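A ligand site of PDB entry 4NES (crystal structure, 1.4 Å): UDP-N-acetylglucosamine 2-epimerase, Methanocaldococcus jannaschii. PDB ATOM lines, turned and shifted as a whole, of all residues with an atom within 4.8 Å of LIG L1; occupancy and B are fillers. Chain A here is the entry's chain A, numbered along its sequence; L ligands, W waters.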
ATOM      1  N   ARG A  10     -27.994  17.161 -15.247  1.00  0.00           N
ATOM      2  CA  ARG A  10     -26.584  16.776 -15.377  1.00  0.00           C
ATOM      3  C   ARG A  10     -25.942  16.976 -16.765  1.00  0.00           C
ATOM      4  O   ARG A  10     -24.952  17.701 -16.870  1.00  0.00           O
ATOM      5  CB  ARG A  10     -26.378  15.330 -14.885  1.00  0.00           C
ATOM      6  CG  ARG A  10     -25.012  14.771 -15.263  1.00  0.00           C
ATOM      7  CD  ARG A  10     -24.791  13.407 -14.610  1.00  0.00           C
ATOM      8  NE  ARG A  10     -25.564  12.326 -15.233  1.00  0.00           N
ATOM      9  CZ  ARG A  10     -25.605  11.085 -14.783  1.00  0.00           C
ATOM     10  NH1 ARG A  10     -24.960  10.747 -13.674  1.00  0.00           N
ATOM     11  NH2 ARG A  10     -26.314  10.174 -15.438  1.00  0.00           N
ATOM     12  N   PRO A  11     -26.487  16.353 -17.825  1.00  0.00           N
ATOM     13  CA  PRO A  11     -25.803  16.509 -19.128  1.00  0.00           C
ATOM     14  C   PRO A  11     -25.798  17.937 -19.655  1.00  0.00           C
ATOM     15  O   PRO A  11     -24.840  18.316 -20.336  1.00  0.00           O
ATOM     16  CB  PRO A  11     -26.631  15.613 -20.058  1.00  0.00           C
ATOM     17  CG  PRO A  11     -27.986  15.510 -19.395  1.00  0.00           C
ATOM     18  CD  PRO A  11     -27.681  15.488 -17.930  1.00  0.00           C
ATOM     19  N   ILE A  14     -22.892  19.939 -18.022  1.00  0.00           N
ATOM     20  CA  ILE A  14     -21.611  19.561 -18.620  1.00  0.00           C
ATOM     21  C   ILE A  14     -21.457  20.193 -20.009  1.00  0.00           C
ATOM     22  O   ILE A  14     -20.431  20.815 -20.307  1.00  0.00           O
ATOM     23  CB  ILE A  14     -21.475  18.023 -18.666  1.00  0.00           C
ATOM     24  CG1 ILE A  14     -21.405  17.453 -17.239  1.00  0.00           C
ATOM     25  CG2 ILE A  14     -20.275  17.609 -19.507  1.00  0.00           C
ATOM     26  CD1 ILE A  14     -21.646  15.961 -17.190  1.00  0.00           C
ATOM     27  N   PHE A  47     -21.371  19.101 -10.317  1.00  0.00           N
ATOM     28  CA  PHE A  47     -20.931  19.602 -11.611  1.00  0.00           C
ATOM     29  C   PHE A  47     -20.642  21.089 -11.580  1.00  0.00           C
ATOM     30  O   PHE A  47     -19.691  21.551 -12.193  1.00  0.00           O
ATOM     31  CB  PHE A  47     -21.950  19.224 -12.688  1.00  0.00           C
ATOM     32  CG  PHE A  47     -22.104  17.749 -12.806  1.00  0.00           C
ATOM     33  CD1 PHE A  47     -21.099  16.985 -13.410  1.00  0.00           C
ATOM     34  CD2 PHE A  47     -23.182  17.094 -12.230  1.00  0.00           C
ATOM     35  CE1 PHE A  47     -21.209  15.614 -13.480  1.00  0.00           C
ATOM     36  CE2 PHE A  47     -23.292  15.723 -12.300  1.00  0.00           C
ATOM     37  CZ  PHE A  47     -22.290  14.987 -12.921  1.00  0.00           C
ATOM     38  N   ASP A  95     -32.115  18.237 -25.093  1.00  0.00           N
ATOM     39  CA  ASP A  95     -33.415  17.644 -25.366  1.00  0.00           C
ATOM     40  C   ASP A  95     -34.233  17.240 -24.124  1.00  0.00           C
ATOM     41  O   ASP A  95     -35.126  16.384 -24.209  1.00  0.00           O
ATOM     42  CB  ASP A  95     -33.224  16.440 -26.277  1.00  0.00           C
ATOM     43  CG  ASP A  95     -32.242  15.433 -25.715  1.00  0.00           C
ATOM     44  OD1 ASP A  95     -32.002  15.454 -24.491  1.00  0.00           O
ATOM     45  OD2 ASP A  95     -31.700  14.636 -26.492  1.00  0.00           O
ATOM     46  N   ILE A 171     -19.412  18.857 -26.229  1.00  0.00           N
ATOM     47  CA  ILE A 171     -18.891  17.780 -25.406  1.00  0.00           C
ATOM     48  C   ILE A 171     -17.418  17.522 -25.730  1.00  0.00           C
ATOM     49  O   ILE A 171     -16.661  17.076 -24.853  1.00  0.00           O
ATOM     50  CB  ILE A 171     -19.735  16.494 -25.534  1.00  0.00           C
ATOM     51  CG1 ILE A 171     -19.434  15.553 -24.370  1.00  0.00           C
ATOM     52  CG2 ILE A 171     -19.513  15.812 -26.883  1.00  0.00           C
ATOM     53  CD1 ILE A 171     -19.804  16.138 -23.039  1.00  0.00           C
ATOM     54  N   THR A 205     -23.777   2.416 -17.985  1.00  0.00           N
ATOM     55  CA  THR A 205     -24.829   3.321 -17.496  1.00  0.00           C
ATOM     56  C   THR A 205     -26.108   3.021 -18.254  1.00  0.00           C
ATOM     57  O   THR A 205     -26.069   2.633 -19.406  1.00  0.00           O
ATOM     58  CB  THR A 205     -24.486   4.840 -17.624  1.00  0.00           C
ATOM     59  OG1 THR A 205     -24.618   5.264 -18.991  1.00  0.00           O
ATOM     60  CG2 THR A 205     -23.095   5.178 -17.072  1.00  0.00           C
ATOM     61  N   HIS A 207     -30.308   4.529 -18.336  1.00  0.00           N
ATOM     62  CA  HIS A 207     -31.383   5.347 -17.764  1.00  0.00           C
ATOM     63  C   HIS A 207     -32.493   5.813 -18.716  1.00  0.00           C
ATOM     64  O   HIS A 207     -33.377   6.547 -18.291  1.00  0.00           O
ATOM     65  CB  HIS A 207     -30.819   6.572 -17.022  1.00  0.00           C
ATOM     66  CG  HIS A 207     -30.365   7.691 -17.914  1.00  0.00           C
ATOM     67  ND1 HIS A 207     -29.114   7.751 -18.464  1.00  0.00           N
ATOM     68  CD2 HIS A 207     -31.020   8.804 -18.328  1.00  0.00           C
ATOM     69  CE1 HIS A 207     -29.001   8.841 -19.193  1.00  0.00           C
ATOM     70  NE2 HIS A 207     -30.150   9.501 -19.127  1.00  0.00           N
ATOM     71  N   ARG A 208     -32.445   5.426 -19.993  1.00  0.00           N
ATOM     72  CA  ARG A 208     -33.512   5.849 -20.923  1.00  0.00           C
ATOM     73  C   ARG A 208     -34.853   5.381 -20.379  1.00  0.00           C
ATOM     74  O   ARG A 208     -34.974   4.242 -19.921  1.00  0.00           O
ATOM     75  CB  ARG A 208     -33.323   5.244 -22.317  1.00  0.00           C
ATOM     76  CG  ARG A 208     -32.103   5.742 -23.096  1.00  0.00           C
ATOM     77  CD  ARG A 208     -32.391   6.971 -23.958  1.00  0.00           C
ATOM     78  NE  ARG A 208     -32.708   8.176 -23.205  1.00  0.00           N
ATOM     79  CZ  ARG A 208     -31.816   8.964 -22.618  1.00  0.00           C
ATOM     80  NH1 ARG A 208     -30.515   8.656 -22.658  1.00  0.00           N
ATOM     81  NH2 ARG A 208     -32.222  10.041 -21.976  1.00  0.00           N
ATOM     82  N   SER A 239     -22.503   2.744 -12.908  1.00  0.00           N
ATOM     83  CA  SER A 239     -22.931   4.004 -12.285  1.00  0.00           C
ATOM     84  C   SER A 239     -24.431   4.107 -12.484  1.00  0.00           C
ATOM     85  O   SER A 239     -24.892   4.216 -13.621  1.00  0.00           O
ATOM     86  CB  SER A 239     -22.236   5.202 -12.934  1.00  0.00           C
ATOM     87  OG  SER A 239     -22.817   6.416 -12.469  1.00  0.00           O
ATOM     88  N   HIS A 241     -28.100   5.642 -12.317  1.00  0.00           N
ATOM     89  CA  HIS A 241     -28.930   6.846 -12.313  1.00  0.00           C
ATOM     90  C   HIS A 241     -30.057   6.657 -11.306  1.00  0.00           C
ATOM     91  O   HIS A 241     -30.554   5.547 -11.143  1.00  0.00           O
ATOM     92  CB  HIS A 241     -29.509   7.000 -13.720  1.00  0.00           C
ATOM     93  CG  HIS A 241     -30.203   8.303 -13.979  1.00  0.00           C
ATOM     94  ND1 HIS A 241     -31.423   8.629 -13.416  1.00  0.00           N
ATOM     95  CD2 HIS A 241     -29.890   9.334 -14.815  1.00  0.00           C
ATOM     96  CE1 HIS A 241     -31.800   9.807 -13.859  1.00  0.00           C
ATOM     97  NE2 HIS A 241     -30.898  10.259 -14.710  1.00  0.00           N
ATOM     98  N   PRO A 268     -23.977   7.810  -8.748  1.00  0.00           N
ATOM     99  CA  PRO A 268     -23.486   8.755  -9.757  1.00  0.00           C
ATOM    100  C   PRO A 268     -22.288   9.549  -9.233  1.00  0.00           C
ATOM    101  O   PRO A 268     -22.282   9.993  -8.077  1.00  0.00           O
ATOM    102  CB  PRO A 268     -24.692   9.674  -9.980  1.00  0.00           C
ATOM    103  CG  PRO A 268     -25.862   8.774  -9.751  1.00  0.00           C
ATOM    104  CD  PRO A 268     -25.444   7.877  -8.610  1.00  0.00           C
ATOM    105  N   VAL A 269     -21.270   9.704 -10.077  1.00  0.00           N
ATOM    106  CA  VAL A 269     -20.052  10.414  -9.692  1.00  0.00           C
ATOM    107  C   VAL A 269     -19.872  11.700 -10.490  1.00  0.00           C
ATOM    108  O   VAL A 269     -20.574  11.951 -11.474  1.00  0.00           O
ATOM    109  CB  VAL A 269     -18.797   9.532  -9.865  1.00  0.00           C
ATOM    110  CG1 VAL A 269     -18.906   8.291  -8.988  1.00  0.00           C
ATOM    111  CG2 VAL A 269     -18.590   9.160 -11.329  1.00  0.00           C
ATOM    112  N   GLY A 270     -18.912  12.527 -10.069  1.00  0.00           N
ATOM    113  CA  GLY A 270     -18.612  13.774 -10.757  1.00  0.00           C
ATOM    114  C   GLY A 270     -18.013  13.543 -12.133  1.00  0.00           C
ATOM    115  O   GLY A 270     -17.626  12.421 -12.474  1.00  0.00           O
ATOM    116  N   TYR A 271     -17.955  14.599 -12.927  1.00  0.00           N
ATOM    117  CA  TYR A 271     -17.475  14.504 -14.302  1.00  0.00           C
ATOM    118  C   TYR A 271     -16.009  14.048 -14.390  1.00  0.00           C
ATOM    119  O   TYR A 271     -15.656  13.232 -15.235  1.00  0.00           O
ATOM    120  CB  TYR A 271     -17.659  15.835 -15.010  1.00  0.00           C
ATOM    121  CG  TYR A 271     -17.484  15.767 -16.509  1.00  0.00           C
ATOM    122  CD1 TYR A 271     -18.135  14.806 -17.253  1.00  0.00           C
ATOM    123  CD2 TYR A 271     -16.686  16.696 -17.171  1.00  0.00           C
ATOM    124  CE1 TYR A 271     -18.001  14.740 -18.626  1.00  0.00           C
ATOM    125  CE2 TYR A 271     -16.547  16.649 -18.557  1.00  0.00           C
ATOM    126  CZ  TYR A 271     -17.210  15.664 -19.269  1.00  0.00           C
ATOM    127  OH  TYR A 271     -17.089  15.601 -20.636  1.00  0.00           O
ATOM    128  N   PHE A 274     -15.878  10.422 -13.627  1.00  0.00           N
ATOM    129  CA  PHE A 274     -16.479   9.613 -14.682  1.00  0.00           C
ATOM    130  C   PHE A 274     -15.607   9.553 -15.927  1.00  0.00           C
ATOM    131  O   PHE A 274     -15.517   8.502 -16.568  1.00  0.00           O
ATOM    132  CB  PHE A 274     -17.904  10.065 -15.006  1.00  0.00           C
ATOM    133  CG  PHE A 274     -18.690   9.013 -15.713  1.00  0.00           C
ATOM    134  CD1 PHE A 274     -19.115   7.890 -15.035  1.00  0.00           C
ATOM    135  CD2 PHE A 274     -18.960   9.118 -17.076  1.00  0.00           C
ATOM    136  CE1 PHE A 274     -19.822   6.889 -15.683  1.00  0.00           C
ATOM    137  CE2 PHE A 274     -19.679   8.119 -17.718  1.00  0.00           C
ATOM    138  CZ  PHE A 274     -20.100   7.009 -17.019  1.00  0.00           C
ATOM    139  N   GLU A 278     -14.398   6.258 -17.876  1.00  0.00           N
ATOM    140  CA  GLU A 278     -14.569   6.034 -19.317  1.00  0.00           C
ATOM    141  C   GLU A 278     -13.244   5.761 -19.995  1.00  0.00           C
ATOM    142  O   GLU A 278     -13.107   4.788 -20.763  1.00  0.00           O
ATOM    143  CB  GLU A 278     -15.222   7.244 -19.972  1.00  0.00           C
ATOM    144  CG  GLU A 278     -16.657   7.477 -19.577  1.00  0.00           C
ATOM    145  CD  GLU A 278     -17.204   8.752 -20.189  1.00  0.00           C
ATOM    146  OE1 GLU A 278     -16.488   9.771 -20.170  1.00  0.00           O
ATOM    147  OE2 GLU A 278     -18.338   8.737 -20.687  1.00  0.00           O
ATOM    148  N   ASP A 287     -26.902   3.474 -22.555  1.00  0.00           N
ATOM    149  CA  ASP A 287     -27.972   4.071 -23.347  1.00  0.00           C
ATOM    150  C   ASP A 287     -27.992   5.594 -23.239  1.00  0.00           C
ATOM    151  O   ASP A 287     -28.957   6.247 -23.636  1.00  0.00           O
ATOM    152  CB  ASP A 287     -29.352   3.451 -23.033  1.00  0.00           C
ATOM    153  CG  ASP A 287     -29.862   3.786 -21.648  1.00  0.00           C
ATOM    154  OD1 ASP A 287     -29.210   4.541 -20.919  1.00  0.00           O
ATOM    155  OD2 ASP A 287     -30.971   3.304 -21.295  1.00  0.00           O
ATOM    156  N   SER A 288     -26.912   6.162 -22.690  1.00  0.00           N
ATOM    157  CA  SER A 288     -26.757   7.615 -22.579  1.00  0.00           C
ATOM    158  C   SER A 288     -26.354   8.260 -23.890  1.00  0.00           C
ATOM    159  O   SER A 288     -25.553   7.692 -24.638  1.00  0.00           O
ATOM    160  CB  SER A 288     -25.666   7.896 -21.547  1.00  0.00           C
ATOM    161  OG  SER A 288     -25.256   9.252 -21.623  1.00  0.00           O
ATOM    162  N   GLY A 289     -26.860   9.458 -24.166  1.00  0.00           N
ATOM    163  CA  GLY A 289     -26.437  10.190 -25.359  1.00  0.00           C
ATOM    164  C   GLY A 289     -25.012  10.707 -25.224  1.00  0.00           C
ATOM    165  O   GLY A 289     -24.174  10.490 -26.110  1.00  0.00           O
ATOM    166  N   GLY A 290     -24.737  11.396 -24.133  1.00  0.00           N
ATOM    167  CA  GLY A 290     -23.413  11.948 -23.909  1.00  0.00           C
ATOM    168  C   GLY A 290     -22.325  10.892 -23.804  1.00  0.00           C
ATOM    169  O   GLY A 290     -21.220  11.111 -24.292  1.00  0.00           O
ATOM    170  N   VAL A 291     -22.632   9.745 -23.201  1.00  0.00           N
ATOM    171  CA  VAL A 291     -21.611   8.714 -23.048  1.00  0.00           C
ATOM    172  C   VAL A 291     -21.229   8.123 -24.415  1.00  0.00           C
ATOM    173  O   VAL A 291     -20.065   7.812 -24.647  1.00  0.00           O
ATOM    174  CB  VAL A 291     -22.025   7.638 -22.044  1.00  0.00           C
ATOM    175  CG1 VAL A 291     -21.009   6.512 -21.992  1.00  0.00           C
ATOM    176  CG2 VAL A 291     -22.188   8.257 -20.664  1.00  0.00           C
ATOM    177  N   GLU A 294     -18.716  10.624 -25.705  1.00  0.00           N
ATOM    178  CA  GLU A 294     -17.452  10.546 -24.979  1.00  0.00           C
ATOM    179  C   GLU A 294     -16.674   9.282 -25.286  1.00  0.00           C
ATOM    180  O   GLU A 294     -15.453   9.324 -25.427  1.00  0.00           O
ATOM    181  CB  GLU A 294     -17.696  10.704 -23.476  1.00  0.00           C
ATOM    182  CG  GLU A 294     -18.159  12.115 -23.170  1.00  0.00           C
ATOM    183  CD  GLU A 294     -18.762  12.275 -21.793  1.00  0.00           C
ATOM    184  OE1 GLU A 294     -19.124  11.261 -21.157  1.00  0.00           O
ATOM    185  OE2 GLU A 294     -18.881  13.431 -21.362  1.00  0.00           O
HETATM  186  N1  LIG L   1     -21.692  11.417 -16.239  1.00  0.00           N
HETATM  187  C1  LIG L   1     -21.067  11.769 -15.092  1.00  0.00           C
HETATM  188  N2  LIG L   1     -21.103  10.932 -14.034  1.00  0.00           N
HETATM  189  C2  LIG L   1     -21.740   9.738 -14.070  1.00  0.00           C
HETATM  190  C3  LIG L   1     -22.389   9.344 -15.249  1.00  0.00           C
HETATM  191  C4  LIG L   1     -22.363  10.229 -16.331  1.00  0.00           C
HETATM  192  O1  LIG L   1     -20.475  12.843 -15.006  1.00  0.00           O
HETATM  193  O2  LIG L   1     -21.743   8.917 -12.950  1.00  0.00           O
HETATM  194  C5  LIG L   1     -21.738  12.306 -17.420  1.00  0.00           C
HETATM  195  C6  LIG L   1     -21.180  11.836 -18.658  1.00  0.00           C
HETATM  196  O3  LIG L   1     -19.781  11.961 -18.650  1.00  0.00           O
HETATM  197  C7  LIG L   1     -21.867  12.661 -19.668  1.00  0.00           C
HETATM  198  C8  LIG L   1     -23.147  12.969 -19.057  1.00  0.00           C
HETATM  199  O4  LIG L   1     -23.111  12.489 -17.731  1.00  0.00           O
HETATM  200  O5  LIG L   1     -21.202  13.852 -19.974  1.00  0.00           O
HETATM  201  C9  LIG L   1     -24.311  12.313 -19.723  1.00  0.00           C
HETATM  202  O6  LIG L   1     -25.508  12.533 -19.026  1.00  0.00           O
HETATM  203  P1  LIG L   1     -26.688  11.463 -18.992  1.00  0.00           P
HETATM  204  O7  LIG L   1     -27.326  11.514 -17.628  1.00  0.00           O
HETATM  205  O8  LIG L   1     -26.138  10.098 -19.332  1.00  0.00           O
HETATM  206  O9  LIG L   1     -27.795  11.928 -20.017  1.00  0.00           O
HETATM  207  P2  LIG L   1     -27.922  11.925 -21.581  1.00  0.00           P
HETATM  208  O10 LIG L   1     -26.589  12.299 -22.216  1.00  0.00           O
HETATM  209  O11 LIG L   1     -28.403  10.561 -22.026  1.00  0.00           O
HETATM  210  O12 LIG L   1     -28.976  12.967 -21.821  1.00  0.00           O
HETATM  211  C1  LG2 L   2     -33.774  13.466 -17.624  1.00  0.00           C
HETATM  212  C2  LG2 L   2     -34.023  13.727 -19.084  1.00  0.00           C
HETATM  213  C3  LG2 L   2     -33.187  12.907 -19.924  1.00  0.00           C
HETATM  214  C4  LG2 L   2     -31.756  13.003 -19.603  1.00  0.00           C
HETATM  215  C5  LG2 L   2     -31.532  12.800 -18.119  1.00  0.00           C
HETATM  216  C6  LG2 L   2     -30.141  13.087 -17.707  1.00  0.00           C
HETATM  217  C7  LG2 L   2     -36.438  14.450 -19.582  1.00  0.00           C
HETATM  218  C8  LG2 L   2     -37.823  14.000 -19.920  1.00  0.00           C
HETATM  219  N1  LG2 L   2     -35.442  13.424 -19.417  1.00  0.00           N
HETATM  220  O1  LG2 L   2     -34.109  12.151 -17.351  1.00  0.00           O
HETATM  221  O2  LG2 L   2     -33.382  13.276 -21.301  1.00  0.00           O
HETATM  222  O3  LG2 L   2     -31.000  12.047 -20.325  1.00  0.00           O
HETATM  223  O4  LG2 L   2     -32.359  13.678 -17.361  1.00  0.00           O
HETATM  224  O5  LG2 L   2     -29.688  12.327 -16.644  1.00  0.00           O
HETATM  225  O6  LG2 L   2     -36.167  15.648 -19.461  1.00  0.00           O
HETATM  226  N2  LG2 L   2     -34.185  11.767  -9.674  1.00  0.00           N
HETATM  227  C9  LG2 L   2     -33.569  11.929  -8.506  1.00  0.00           C
HETATM  228  N3  LG2 L   2     -32.762  12.974  -8.313  1.00  0.00           N
HETATM  229  C10 LG2 L   2     -32.566  13.900  -9.263  1.00  0.00           C
HETATM  230  C11 LG2 L   2     -33.201  13.761 -10.495  1.00  0.00           C
HETATM  231  C12 LG2 L   2     -34.022  12.656 -10.692  1.00  0.00           C
HETATM  232  O7  LG2 L   2     -33.708  11.121  -7.612  1.00  0.00           O
HETATM  233  O8  LG2 L   2     -31.747  14.958  -9.037  1.00  0.00           O
HETATM  234  C13 LG2 L   2     -35.066  10.611  -9.923  1.00  0.00           C
HETATM  235  C14 LG2 L   2     -36.461  10.776  -9.471  1.00  0.00           C
HETATM  236  O9  LG2 L   2     -36.952   9.550  -8.997  1.00  0.00           O
HETATM  237  C15 LG2 L   2     -37.156  11.168 -10.671  1.00  0.00           C
HETATM  238  C16 LG2 L   2     -36.479  10.348 -11.700  1.00  0.00           C
HETATM  239  O10 LG2 L   2     -35.112  10.288 -11.317  1.00  0.00           O
HETATM  240  O11 LG2 L   2     -38.543  10.956 -10.637  1.00  0.00           O
HETATM  241  C17 LG2 L   2     -36.580  10.931 -13.065  1.00  0.00           C
HETATM  242  O12 LG2 L   2     -36.183  12.285 -13.166  1.00  0.00           O
HETATM  243  P1  LG2 L   2     -36.472  13.083 -14.461  1.00  0.00           P
HETATM  244  O13 LG2 L   2     -37.946  13.129 -14.683  1.00  0.00           O
HETATM  245  O14 LG2 L   2     -35.879  14.450 -14.321  1.00  0.00           O
HETATM  246  O15 LG2 L   2     -35.876  12.306 -15.683  1.00  0.00           O
HETATM  247  P2  LG2 L   2     -34.437  11.663 -15.884  1.00  0.00           P
HETATM  248  O16 LG2 L   2     -34.601  10.178 -15.940  1.00  0.00           O
HETATM  249  O17 LG2 L   2     -33.448  12.196 -14.878  1.00  0.00           O
HETATM  250  O   HOH W   1     -23.397  12.124 -11.809  1.00  0.00           O
HETATM  251  O   HOH W   2     -24.797   8.172 -17.964  1.00  0.00           O
HETATM  252  O   HOH W   3     -25.239  14.485 -22.891  1.00  0.00           O
HETATM  253  O   HOH W   4     -23.235  15.594 -21.263  1.00  0.00           O
HETATM  254  O   HOH W   5     -31.263  13.363 -23.124  1.00  0.00           O
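Merely in contact with LIG L1: Pro 11, Ile 14, Phe 47, Pro 268, Gly 270, Tyr 271 and Phe 274.
Hydrophobic or aromatic side chains that line LIG L1: Pro 11, Ile 14, Phe 47, His 207, Val 269, Tyr 271 and Phe 274.
Of the 23 residues printed, 16 come within 4 Å of LIG L1.
OG of Ser 288 is in hydrogen-bond range of O8 of LIG L1 (2.6 Å).
An oxygen (O3) of LIG L1 lies within hydrogen-bond range of the side-chain carboxylate (OE1) of Glu 294 (2.7 Å).
NH2 of Arg 10 is in salt-bridge range of O7 of LIG L1, at 2.8 Å.
An oxygen (O2) of LIG L1 is in hydrogen-bond range of the side-chain hydroxyl of Ser 239 (2.8 Å).
The backbone NH (N) of Val 269 sits at hydrogen-bond distance from an oxygen (O2) of LIG L1 (3.0 Å).
The backbone carbonyl oxygen (O) of Val 269 sits at hydrogen-bond distance from a nitrogen (N2) of LIG L1.
N of Gly 290 is in hydrogen-bond range of O10 of LIG L1.
O11 of LIG L1 lies within hydrogen-bond range of N of Gly 289, 2.9 Å away.
NH1 of Arg 208 lies within salt-bridge range of O11 of LIG L1 (2.9 Å).
O9 of LIG L1 lies close to NE2 of His 207, at 3.5 Å.
NH2 of Arg 208 is in hydrogen-bond range of O3 of LG2 L2, at 2.9 Å.
A ring nitrogen (NE2) of His 207 lies within hydrogen-bond range of an oxygen (O3) of LG2 L2, at 2.9 Å.
A ring nitrogen (NE2) of His 241 lies within hydrogen-bond range of an oxygen (O5) of LG2 L2.
An oxygen (O3) of LG2 L2 is in hydrogen-bond range of an oxygen (O12) of LIG L1.
Water W3 lies within hydrogen-bond range of O10 of LIG L1 (2.7 Å) and N of Gly 290 (3.4 Å).
Water W5 lies within hydrogen-bond range of OD1 of Asp 95 (2.6 Å), O12 of LIG L1 (2.7 Å) and O2 of LG2 L2 (2.8 Å).
Water W2 lies within hydrogen-bond range of O8 of LIG L1 (2.7 Å) and OG1 of Thr 205 (3.1 Å).
Water W4 bridges O5 of LIG L1 and O of Pro 11.
Water W1 lies within hydrogen-bond range of NH1 of Arg 10 (2.8 Å), O of Val 269 (2.8 Å) and N2 of LIG L1 (3.4 Å).
The side-chain hydroxyl of Ser 288 sits at hydrogen-bond distance from the backbone NH of Gly 290.
The backbone NH (N) of Val 291 lies within hydrogen-bond range of the side-chain hydroxyl (OG) of Ser 288 (3.1 Å).
OE2 of Glu 294 is in hydrogen-bond range of OH of Tyr 271.
The side-chain carboxylate (OE1) of Glu 294 lies close to the side-chain carboxylate (OE2) of Glu 278.
The side-chain carboxylate (OD2) of Asp 287 sits at hydrogen-bond distance from the backbone NH (N) of Arg 208, 2.9 Å away.
The backbone NH of His 207 lies within hydrogen-bond range of the side-chain carboxylate of Asp 287 (2.8 Å).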
